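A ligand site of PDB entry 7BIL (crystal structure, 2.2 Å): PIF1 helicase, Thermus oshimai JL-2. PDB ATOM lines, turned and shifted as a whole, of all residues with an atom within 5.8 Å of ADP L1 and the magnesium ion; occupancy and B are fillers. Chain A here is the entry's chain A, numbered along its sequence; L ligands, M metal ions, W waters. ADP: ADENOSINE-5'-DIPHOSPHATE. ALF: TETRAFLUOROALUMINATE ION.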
ATOM      1  N   GLY A  67      16.500  24.872  -3.353  1.00  0.00           N
ATOM      2  CA  GLY A  67      15.447  23.926  -3.708  1.00  0.00           C
ATOM      3  C   GLY A  67      14.390  24.524  -4.627  1.00  0.00           C
ATOM      4  O   GLY A  67      14.324  25.730  -4.826  1.00  0.00           O
ATOM      5  N   LEU A  68      13.551  23.654  -5.145  1.00  0.00           N
ATOM      6  CA  LEU A  68      12.543  24.036  -6.116  1.00  0.00           C
ATOM      7  C   LEU A  68      11.461  24.869  -5.471  1.00  0.00           C
ATOM      8  O   LEU A  68      11.186  24.721  -4.291  1.00  0.00           O
ATOM      9  CB  LEU A  68      11.928  22.783  -6.736  1.00  0.00           C
ATOM     10  CG  LEU A  68      12.909  21.882  -7.498  1.00  0.00           C
ATOM     11  CD1 LEU A  68      12.236  20.553  -7.951  1.00  0.00           C
ATOM     12  CD2 LEU A  68      13.509  22.651  -8.672  1.00  0.00           C
ATOM     13  N   SER A  69      10.846  25.743  -6.254  1.00  0.00           N
ATOM     14  CA  SER A  69       9.637  26.402  -5.772  1.00  0.00           C
ATOM     15  C   SER A  69       8.491  25.400  -5.761  1.00  0.00           C
ATOM     16  O   SER A  69       8.578  24.324  -6.367  1.00  0.00           O
ATOM     17  CB  SER A  69       9.245  27.531  -6.696  1.00  0.00           C
ATOM     18  OG  SER A  69       8.919  27.029  -7.985  1.00  0.00           O
ATOM     19  N   GLN A  72       7.372  24.317  -9.161  1.00  0.00           N
ATOM     20  CA  GLN A  72       8.360  23.444  -9.804  1.00  0.00           C
ATOM     21  C   GLN A  72       8.256  22.039  -9.215  1.00  0.00           C
ATOM     22  O   GLN A  72       8.422  21.033  -9.919  1.00  0.00           O
ATOM     23  CB  GLN A  72       9.782  24.003  -9.611  1.00  0.00           C
ATOM     24  CG  GLN A  72      10.185  25.212 -10.448  1.00  0.00           C
ATOM     25  CD  GLN A  72      11.543  25.764  -9.982  1.00  0.00           C
ATOM     26  OE1 GLN A  72      11.783  25.914  -8.785  1.00  0.00           O
ATOM     27  NE2 GLN A  72      12.435  26.017 -10.928  1.00  0.00           N
ATOM     28  N   GLY A  91       6.222  27.631 -19.705  1.00  0.00           N
ATOM     29  CA  GLY A  91       6.026  28.844 -18.962  1.00  0.00           C
ATOM     30  C   GLY A  91       6.941  29.937 -19.472  1.00  0.00           C
ATOM     31  O   GLY A  91       7.912  29.677 -20.211  1.00  0.00           O
ATOM     32  N   PRO A  92       6.675  31.182 -19.047  1.00  0.00           N
ATOM     33  CA  PRO A  92       7.490  32.329 -19.490  1.00  0.00           C
ATOM     34  C   PRO A  92       8.977  32.172 -19.174  1.00  0.00           C
ATOM     35  O   PRO A  92       9.450  31.284 -18.445  1.00  0.00           O
ATOM     36  CB  PRO A  92       6.878  33.543 -18.752  1.00  0.00           C
ATOM     37  CG  PRO A  92       5.546  33.086 -18.263  1.00  0.00           C
ATOM     38  CD  PRO A  92       5.642  31.559 -18.068  1.00  0.00           C
ATOM     39  N   ALA A  93       9.737  33.057 -19.798  1.00  0.00           N
ATOM     40  CA  ALA A  93      11.184  33.022 -19.696  1.00  0.00           C
ATOM     41  C   ALA A  93      11.598  33.135 -18.228  1.00  0.00           C
ATOM     42  O   ALA A  93      11.050  33.956 -17.483  1.00  0.00           O
ATOM     43  CB  ALA A  93      11.760  34.177 -20.503  1.00  0.00           C
ATOM     44  N   GLY A  94      12.515  32.283 -17.782  1.00  0.00           N
ATOM     45  CA  GLY A  94      13.038  32.425 -16.413  1.00  0.00           C
ATOM     46  C   GLY A  94      12.150  31.943 -15.284  1.00  0.00           C
ATOM     47  O   GLY A  94      12.414  32.237 -14.116  1.00  0.00           O
ATOM     48  N   THR A  95      11.136  31.130 -15.571  1.00  0.00           N
ATOM     49  CA  THR A  95      10.307  30.518 -14.548  1.00  0.00           C
ATOM     50  C   THR A  95      11.008  29.305 -13.900  1.00  0.00           C
ATOM     51  O   THR A  95      10.499  28.728 -12.943  1.00  0.00           O
ATOM     52  CB  THR A  95       8.931  30.180 -15.149  1.00  0.00           C
ATOM     53  OG1 THR A  95       9.136  29.532 -16.410  1.00  0.00           O
ATOM     54  CG2 THR A  95       8.102  31.486 -15.413  1.00  0.00           C
ATOM     55  N   GLY A  96      12.162  28.891 -14.421  1.00  0.00           N
ATOM     56  CA  GLY A  96      12.891  27.813 -13.813  1.00  0.00           C
ATOM     57  C   GLY A  96      12.674  26.472 -14.469  1.00  0.00           C
ATOM     58  O   GLY A  96      12.749  25.439 -13.794  1.00  0.00           O
ATOM     59  N   LYS A  97      12.427  26.463 -15.770  1.00  0.00           N
ATOM     60  CA  LYS A  97      12.203  25.244 -16.531  1.00  0.00           C
ATOM     61  C   LYS A  97      13.461  24.396 -16.540  1.00  0.00           C
ATOM     62  O   LYS A  97      13.451  23.239 -16.126  1.00  0.00           O
ATOM     63  CB  LYS A  97      11.764  25.628 -17.940  1.00  0.00           C
ATOM     64  CG  LYS A  97      10.362  26.223 -17.918  1.00  0.00           C
ATOM     65  CD  LYS A  97       9.819  26.555 -19.307  1.00  0.00           C
ATOM     66  CE  LYS A  97      10.764  27.498 -20.020  1.00  0.00           C
ATOM     67  NZ  LYS A  97      10.859  28.821 -19.283  1.00  0.00           N
ATOM     68  N   THR A  98      14.585  25.002 -16.897  1.00  0.00           N
ATOM     69  CA  THR A  98      15.844  24.281 -16.962  1.00  0.00           C
ATOM     70  C   THR A  98      16.328  23.879 -15.576  1.00  0.00           C
ATOM     71  O   THR A  98      16.955  22.826 -15.417  1.00  0.00           O
ATOM     72  CB  THR A  98      16.856  25.128 -17.728  1.00  0.00           C
ATOM     73  OG1 THR A  98      16.374  25.293 -19.056  1.00  0.00           O
ATOM     74  CG2 THR A  98      18.223  24.436 -17.778  1.00  0.00           C
ATOM     75  N   THR A  99      16.048  24.683 -14.566  1.00  0.00           N
ATOM     76  CA  THR A  99      16.408  24.303 -13.199  1.00  0.00           C
ATOM     77  C   THR A  99      15.597  23.084 -12.749  1.00  0.00           C
ATOM     78  O   THR A  99      16.106  22.190 -12.068  1.00  0.00           O
ATOM     79  CB  THR A  99      16.212  25.496 -12.265  1.00  0.00           C
ATOM     80  OG1 THR A  99      17.177  26.521 -12.596  1.00  0.00           O
ATOM     81  CG2 THR A  99      16.436  25.106 -10.789  1.00  0.00           C
ATOM     82  N   LEU A 100      14.325  23.026 -13.131  1.00  0.00           N
ATOM     83  CA  LEU A 100      13.539  21.835 -12.858  1.00  0.00           C
ATOM     84  C   LEU A 100      14.113  20.657 -13.648  1.00  0.00           C
ATOM     85  O   LEU A 100      14.173  19.531 -13.148  1.00  0.00           O
ATOM     86  CB  LEU A 100      12.053  22.104 -13.185  1.00  0.00           C
ATOM     87  CG  LEU A 100      11.129  20.898 -13.361  1.00  0.00           C
ATOM     88  CD1 LEU A 100      11.180  20.020 -12.126  1.00  0.00           C
ATOM     89  CD2 LEU A 100       9.718  21.348 -13.596  1.00  0.00           C
ATOM     90  N   GLN A 124      23.580  24.588 -21.461  1.00  0.00           N
ATOM     91  CA  GLN A 124      22.839  25.118 -20.312  1.00  0.00           C
ATOM     92  C   GLN A 124      22.051  23.997 -19.636  1.00  0.00           C
ATOM     93  O   GLN A 124      21.901  23.994 -18.399  1.00  0.00           O
ATOM     94  CB  GLN A 124      21.906  26.252 -20.762  1.00  0.00           C
ATOM     95  CG  GLN A 124      20.979  26.790 -19.688  1.00  0.00           C
ATOM     96  CD  GLN A 124      21.706  27.683 -18.694  1.00  0.00           C
ATOM     97  OE1 GLN A 124      22.669  28.347 -19.039  1.00  0.00           O
ATOM     98  NE2 GLN A 124      21.287  27.649 -17.442  1.00  0.00           N
ATOM     99  N   ASP A 171      14.989  20.039 -23.838  1.00  0.00           N
ATOM    100  CA  ASP A 171      14.862  21.433 -23.404  1.00  0.00           C
ATOM    101  C   ASP A 171      14.766  22.399 -24.608  1.00  0.00           C
ATOM    102  O   ASP A 171      15.113  22.059 -25.741  1.00  0.00           O
ATOM    103  CB  ASP A 171      16.035  21.818 -22.474  1.00  0.00           C
ATOM    104  CG  ASP A 171      15.705  23.060 -21.515  1.00  0.00           C
ATOM    105  OD1 ASP A 171      14.545  23.538 -21.536  1.00  0.00           O
ATOM    106  OD2 ASP A 171      16.595  23.513 -20.750  1.00  0.00           O
ATOM    107  N   GLU A 172      14.311  23.610 -24.343  1.00  0.00           N
ATOM    108  CA  GLU A 172      14.077  24.610 -25.390  1.00  0.00           C
ATOM    109  C   GLU A 172      13.307  24.059 -26.589  1.00  0.00           C
ATOM    110  O   GLU A 172      13.627  24.336 -27.755  1.00  0.00           O
ATOM    111  CB  GLU A 172      15.391  25.233 -25.826  1.00  0.00           C
ATOM    112  CG  GLU A 172      15.983  26.171 -24.785  1.00  0.00           C
ATOM    113  CD  GLU A 172      15.105  27.424 -24.421  1.00  0.00           C
ATOM    114  OE1 GLU A 172      15.643  28.196 -23.617  1.00  0.00           O
ATOM    115  OE2 GLU A 172      13.921  27.604 -24.881  1.00  0.00           O
ATOM    116  N   GLN A 212       9.016  32.250 -27.150  1.00  0.00           N
ATOM    117  CA  GLN A 212      10.415  32.496 -27.443  1.00  0.00           C
ATOM    118  C   GLN A 212      10.669  32.077 -28.882  1.00  0.00           C
ATOM    119  O   GLN A 212       9.736  31.927 -29.662  1.00  0.00           O
ATOM    120  CB  GLN A 212      11.312  31.845 -26.397  1.00  0.00           C
ATOM    121  CG  GLN A 212      11.081  32.517 -24.977  1.00  0.00           C
ATOM    122  CD  GLN A 212      12.010  31.966 -23.916  1.00  0.00           C
ATOM    123  OE1 GLN A 212      13.235  31.863 -24.130  1.00  0.00           O
ATOM    124  NE2 GLN A 212      11.430  31.620 -22.758  1.00  0.00           N
ATOM    125  N   LEU A 251       4.403  26.694 -15.525  1.00  0.00           N
ATOM    126  CA  LEU A 251       5.088  27.472 -14.484  1.00  0.00           C
ATOM    127  C   LEU A 251       4.796  28.964 -14.718  1.00  0.00           C
ATOM    128  O   LEU A 251       4.755  29.411 -15.865  1.00  0.00           O
ATOM    129  CB  LEU A 251       6.599  27.256 -14.479  1.00  0.00           C
ATOM    130  CG  LEU A 251       7.115  25.814 -14.451  1.00  0.00           C
ATOM    131  CD1 LEU A 251       8.640  25.810 -14.452  1.00  0.00           C
ATOM    132  CD2 LEU A 251       6.555  25.054 -13.267  1.00  0.00           C
ATOM    133  N   GLN A 255      11.522  33.357 -11.729  1.00  0.00           N
ATOM    134  CA  GLN A 255      12.640  33.104 -10.846  1.00  0.00           C
ATOM    135  C   GLN A 255      13.827  33.968 -11.189  1.00  0.00           C
ATOM    136  O   GLN A 255      14.550  34.419 -10.297  1.00  0.00           O
ATOM    137  CB  GLN A 255      13.044  31.610 -10.893  1.00  0.00           C
ATOM    138  CG  GLN A 255      11.940  30.704 -10.454  1.00  0.00           C
ATOM    139  CD  GLN A 255      11.495  30.882  -9.002  1.00  0.00           C
ATOM    140  OE1 GLN A 255      12.281  31.264  -8.130  1.00  0.00           O
ATOM    141  NE2 GLN A 255      10.223  30.598  -8.738  1.00  0.00           N
ATOM    142  N   ARG A 256      14.065  34.168 -12.486  1.00  0.00           N
ATOM    143  CA  ARG A 256      15.178  34.986 -12.952  1.00  0.00           C
ATOM    144  C   ARG A 256      15.006  36.425 -12.469  1.00  0.00           C
ATOM    145  O   ARG A 256      15.977  37.088 -12.095  1.00  0.00           O
ATOM    146  CB  ARG A 256      15.281  34.929 -14.493  1.00  0.00           C
ATOM    147  CG  ARG A 256      16.429  35.829 -15.080  1.00  0.00           C
ATOM    148  CD  ARG A 256      16.676  35.576 -16.575  1.00  0.00           C
ATOM    149  NE  ARG A 256      17.051  34.206 -16.853  1.00  0.00           N
ATOM    150  CZ  ARG A 256      16.484  33.416 -17.776  1.00  0.00           C
ATOM    151  NH1 ARG A 256      15.546  33.904 -18.609  1.00  0.00           N
ATOM    152  NH2 ARG A 256      16.914  32.172 -17.910  1.00  0.00           N
ATOM    153  N   ARG A 258      13.019  37.362  -9.930  1.00  0.00           N
ATOM    154  CA  ARG A 258      12.366  37.303  -8.623  1.00  0.00           C
ATOM    155  C   ARG A 258      12.647  38.546  -7.796  1.00  0.00           C
ATOM    156  O   ARG A 258      11.754  39.063  -7.115  1.00  0.00           O
ATOM    157  CB  ARG A 258      12.855  36.061  -7.875  1.00  0.00           C
ATOM    158  CG  ARG A 258      12.227  35.789  -6.553  1.00  0.00           C
ATOM    159  CD  ARG A 258      12.675  34.408  -6.021  1.00  0.00           C
ATOM    160  NE  ARG A 258      14.122  34.273  -5.929  1.00  0.00           N
ATOM    161  CZ  ARG A 258      14.766  33.294  -5.299  1.00  0.00           C
ATOM    162  NH1 ARG A 258      14.073  32.319  -4.683  1.00  0.00           N
ATOM    163  NH2 ARG A 258      16.103  33.286  -5.263  1.00  0.00           N
ATOM    164  N   GLY A 436      18.040  30.767 -23.369  1.00  0.00           N
ATOM    165  CA  GLY A 436      18.332  29.816 -22.321  1.00  0.00           C
ATOM    166  C   GLY A 436      19.289  30.320 -21.266  1.00  0.00           C
ATOM    167  O   GLY A 436      19.371  29.730 -20.191  1.00  0.00           O
ATOM    168  N   THR A 438      21.050  32.964 -18.519  1.00  0.00           N
ATOM    169  CA  THR A 438      20.877  34.102 -17.635  1.00  0.00           C
ATOM    170  C   THR A 438      22.145  34.933 -17.746  1.00  0.00           C
ATOM    171  O   THR A 438      23.238  34.406 -17.538  1.00  0.00           O
ATOM    172  CB  THR A 438      20.676  33.636 -16.198  1.00  0.00           C
ATOM    173  OG1 THR A 438      19.414  32.999 -16.121  1.00  0.00           O
ATOM    174  CG2 THR A 438      20.613  34.824 -15.217  1.00  0.00           C
ATOM    175  N   ARG A 462      16.703  38.023 -20.622  1.00  0.00           N
ATOM    176  CA  ARG A 462      17.934  37.363 -20.196  1.00  0.00           C
ATOM    177  C   ARG A 462      18.437  37.826 -18.817  1.00  0.00           C
ATOM    178  O   ARG A 462      19.176  37.085 -18.171  1.00  0.00           O
ATOM    179  CB  ARG A 462      19.030  37.574 -21.231  1.00  0.00           C
ATOM    180  CG  ARG A 462      18.689  37.113 -22.637  1.00  0.00           C
ATOM    181  CD  ARG A 462      18.324  35.621 -22.682  1.00  0.00           C
ATOM    182  NE  ARG A 462      16.889  35.372 -22.557  1.00  0.00           N
ATOM    183  CZ  ARG A 462      16.390  34.255 -22.023  1.00  0.00           C
ATOM    184  NH1 ARG A 462      17.243  33.330 -21.550  1.00  0.00           N
ATOM    185  NH2 ARG A 462      15.085  34.038 -21.928  1.00  0.00           N
ATOM    186  N   ARG A 464      18.335  39.753 -14.787  1.00  0.00           N
ATOM    187  CA  ARG A 464      17.554  39.702 -13.558  1.00  0.00           C
ATOM    188  C   ARG A 464      16.879  41.008 -13.230  1.00  0.00           C
ATOM    189  O   ARG A 464      15.854  41.003 -12.545  1.00  0.00           O
ATOM    190  CB  ARG A 464      18.468  39.261 -12.392  1.00  0.00           C
ATOM    191  CG  ARG A 464      19.186  37.859 -12.662  1.00  0.00           C
ATOM    192  CD  ARG A 464      20.209  37.584 -11.558  1.00  0.00           C
ATOM    193  NE  ARG A 464      21.041  36.392 -11.827  1.00  0.00           N
ATOM    194  CZ  ARG A 464      22.117  36.409 -12.631  1.00  0.00           C
ATOM    195  NH1 ARG A 464      22.461  37.544 -13.233  1.00  0.00           N
ATOM    196  NH2 ARG A 464      22.840  35.312 -12.834  1.00  0.00           N
HETATM  197  PB  ADP L   1      14.043  28.990 -17.663  1.00  0.00           P
HETATM  198  O1B ADP L   1      12.626  28.885 -17.276  1.00  0.00           O
HETATM  199  O2B ADP L   1      14.725  27.656 -18.116  1.00  0.00           O
HETATM  200  O3B ADP L   1      14.171  30.132 -18.630  1.00  0.00           O
HETATM  201  PA  ADP L   1      16.093  28.819 -15.530  1.00  0.00           P
HETATM  202  O1A ADP L   1      15.792  27.414 -14.931  1.00  0.00           O
HETATM  203  O2A ADP L   1      17.324  29.013 -16.393  1.00  0.00           O
HETATM  204  O3A ADP L   1      14.751  29.343 -16.301  1.00  0.00           O
HETATM  205  O5' ADP L   1      16.122  29.828 -14.268  1.00  0.00           O
HETATM  206  C5' ADP L   1      16.415  31.222 -14.442  1.00  0.00           C
HETATM  207  C4' ADP L   1      17.262  31.766 -13.282  1.00  0.00           C
HETATM  208  O4' ADP L   1      16.587  31.630 -12.006  1.00  0.00           O
HETATM  209  C3' ADP L   1      18.526  30.937 -13.173  1.00  0.00           C
HETATM  210  O3' ADP L   1      19.600  31.804 -12.735  1.00  0.00           O
HETATM  211  C2' ADP L   1      18.226  29.876 -12.107  1.00  0.00           C
HETATM  212  O2' ADP L   1      19.377  29.504 -11.343  1.00  0.00           O
HETATM  213  C1' ADP L   1      17.317  30.662 -11.193  1.00  0.00           C
HETATM  214  N9  ADP L   1      16.304  29.771 -10.602  1.00  0.00           N
HETATM  215  C8  ADP L   1      15.405  28.975 -11.258  1.00  0.00           C
HETATM  216  N7  ADP L   1      14.583  28.365 -10.356  1.00  0.00           N
HETATM  217  C5  ADP L   1      14.971  28.732  -9.115  1.00  0.00           C
HETATM  218  C6  ADP L   1      14.562  28.471  -7.711  1.00  0.00           C
HETATM  219  N6  ADP L   1      13.545  27.640  -7.411  1.00  0.00           N
HETATM  220  N1  ADP L   1      15.221  29.113  -6.721  1.00  0.00           N
HETATM  221  C2  ADP L   1      16.236  29.968  -6.951  1.00  0.00           C
HETATM  222  N3  ADP L   1      16.665  30.262  -8.194  1.00  0.00           N
HETATM  223  C4  ADP L   1      16.084  29.680  -9.285  1.00  0.00           C
HETATM  224 AL   ALF L   2      14.506  30.353 -20.543  1.00  0.00          AL
HETATM  225  F1  ALF L   2      14.009  32.061 -20.318  1.00  0.00           F
HETATM  226  F2  ALF L   2      14.976  28.647 -20.781  1.00  0.00           F
HETATM  227  F3  ALF L   2      12.772  29.915 -20.730  1.00  0.00           F
HETATM  228  F4  ALF L   2      16.174  30.802 -20.162  1.00  0.00           F
HETATM  229 MG    MG M   1      15.696  27.265 -19.754  1.00  0.00          MG
HETATM  230  O   HOH W   1      22.108  31.023 -13.338  1.00  0.00           O
HETATM  231  O   HOH W   2      19.490  26.666 -11.905  1.00  0.00           O
HETATM  232  O   HOH W   3      14.309  26.081 -20.728  1.00  0.00           O
HETATM  233  O   HOH W   4      16.872  26.965 -21.409  1.00  0.00           O
HETATM  234  O   HOH W   5      20.889  31.244  -9.794  1.00  0.00           O
HETATM  235  O   HOH W   6      17.380  28.086 -18.976  1.00  0.00           O
HETATM  236  O   HOH W   7      19.139  34.345 -11.195  1.00  0.00           O
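The magnesium ion is bound by a fluorine (F2) of ALF L2 (1.9 Å). O2B of ADP L1 binds the magnesium ion, 1.9 Å away. The magnesium ion is bound by water W6 (2.0 Å). The magnesium ion is bound by water W4 (2.1 Å). Water W3 is bound to the magnesium ion. The magnesium ion is bound by the side-chain hydroxyl (OG1) of Thr 98.
Merely in contact with the magnesium ion: Glu 172 (3.97 Å) and Asp 171 (3.98 Å). Of the 26 residues printed, 3 come within 4 Å of the magnesium ion.
The backbone NH of Thr 98 is in hydrogen-bond range of an oxygen (O1A) of ADP L1 (3.3 Å). N of Lys 97 lies within hydrogen-bond range of O1B of ADP L1 (2.9 Å). The side-chain amino group (NZ) of Lys 97 is in salt-bridge range of an oxygen (O1B) of ADP L1. O1A of ADP L1 sits at hydrogen-bond distance from N of Thr 99, 2.8 Å away. OG1 of Thr 99 lies within hydrogen-bond range of O1A of ADP L1. A nitrogen (N6) of ADP L1 is in hydrogen-bond range of the side-chain amide oxygen (OE1) of Gln 72 (2.8 Å). The backbone NH (N) of Gly 94 sits at hydrogen-bond distance from an oxygen (O1B) of ADP L1 (3.4 Å). N of Gly 96 is in hydrogen-bond range of O1B of ADP L1 (2.9 Å). An oxygen (O1B) of ADP L1 is in hydrogen-bond range of the backbone NH of Thr 95 (3.2 Å). The backbone carbonyl oxygen (O) of Gly 67 is in hydrogen-bond range of a nitrogen (N6) of ADP L1 (3.3 Å). An oxygen (O2A) of ADP L1 is in salt-bridge range of the guanidinium group (NH2) of Arg 256 (3.5 Å). The side-chain amino group (NZ) of Lys 97 sits at hydrogen-bond distance from a fluorine (F3) of ALF L2. N of Gly 94 is in hydrogen-bond range of F1 of ALF L2 (3.0 Å). The guanidinium group of Arg 256 sits at hydrogen-bond distance from a fluorine (F4) of ALF L2 (2.7 Å). F3 of ALF L2 sits at hydrogen-bond distance from NE2 of Gln 212. The guanidinium group of Arg 462 lies within hydrogen-bond range of a fluorine (F1) of ALF L2, 2.8 Å away.
AL of ALF L2 is bound by O3B of ADP L1 (2.0 Å).
The side-chain carboxylate of Asp 171 lies close to the side-chain hydroxyl of Thr 98. The backbone carbonyl oxygen (O) of Gly 91 sits at hydrogen-bond distance from the side-chain amino group (NZ) of Lys 97 (3.2 Å). The side-chain amide nitrogen (NE2) of Gln 72 is in hydrogen-bond range of the backbone carbonyl oxygen (O) of Gly 96 (2.9 Å). The side-chain amide oxygen (OE1) of Gln 72 sits at hydrogen-bond distance from the backbone NH (N) of Ser 69 (2.7 Å). O of Gly 94 lies within hydrogen-bond range of N of Arg 256 (3.0 Å). N of Gln 255 lies within hydrogen-bond range of O of Gly 94, 2.8 Å away. The side-chain hydroxyl (OG1) of Thr 95 lies within hydrogen-bond range of the backbone carbonyl oxygen (O) of Pro 92 (2.7 Å). The guanidinium group (NE) of Arg 256 lies within hydrogen-bond range of the side-chain hydroxyl (OG1) of Thr 438 (2.8 Å).
The backbone NH (N) of Ser 69 sits close to a nitrogen (N6) of ADP L1 (3.5 Å). Leu 68 touches ADP L1 (CA to N6, 3.96 Å). Ala 93 touches ADP L1. Gln 255 touches ADP L1. Arg 258 touches ADP L1 (NH2 to C2, 3.7 Å). Thr 438 touches ADP L1. 15 residues have an atom within 4 Å of ADP L1: Gly 67, Leu 68, Ser 69, Gln 72, Ala 93, Gly 94, Thr 95, Gly 96, Lys 97, Thr 98, Thr 99, Gln 255, Arg 256, Arg 258 and Thr 438.
Water W6 bridges an oxygen (O2A) of ADP L1 (2.7 Å) and the backbone carbonyl oxygen of Gly 436 (2.9 Å). Water W2 bridges OG1 of Thr 99 and O2' of ADP L1. Water W7 bridges the guanidinium group (NE) of Arg 464 (2.9 Å) and an oxygen (O3') of ADP L1 (3.0 Å).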
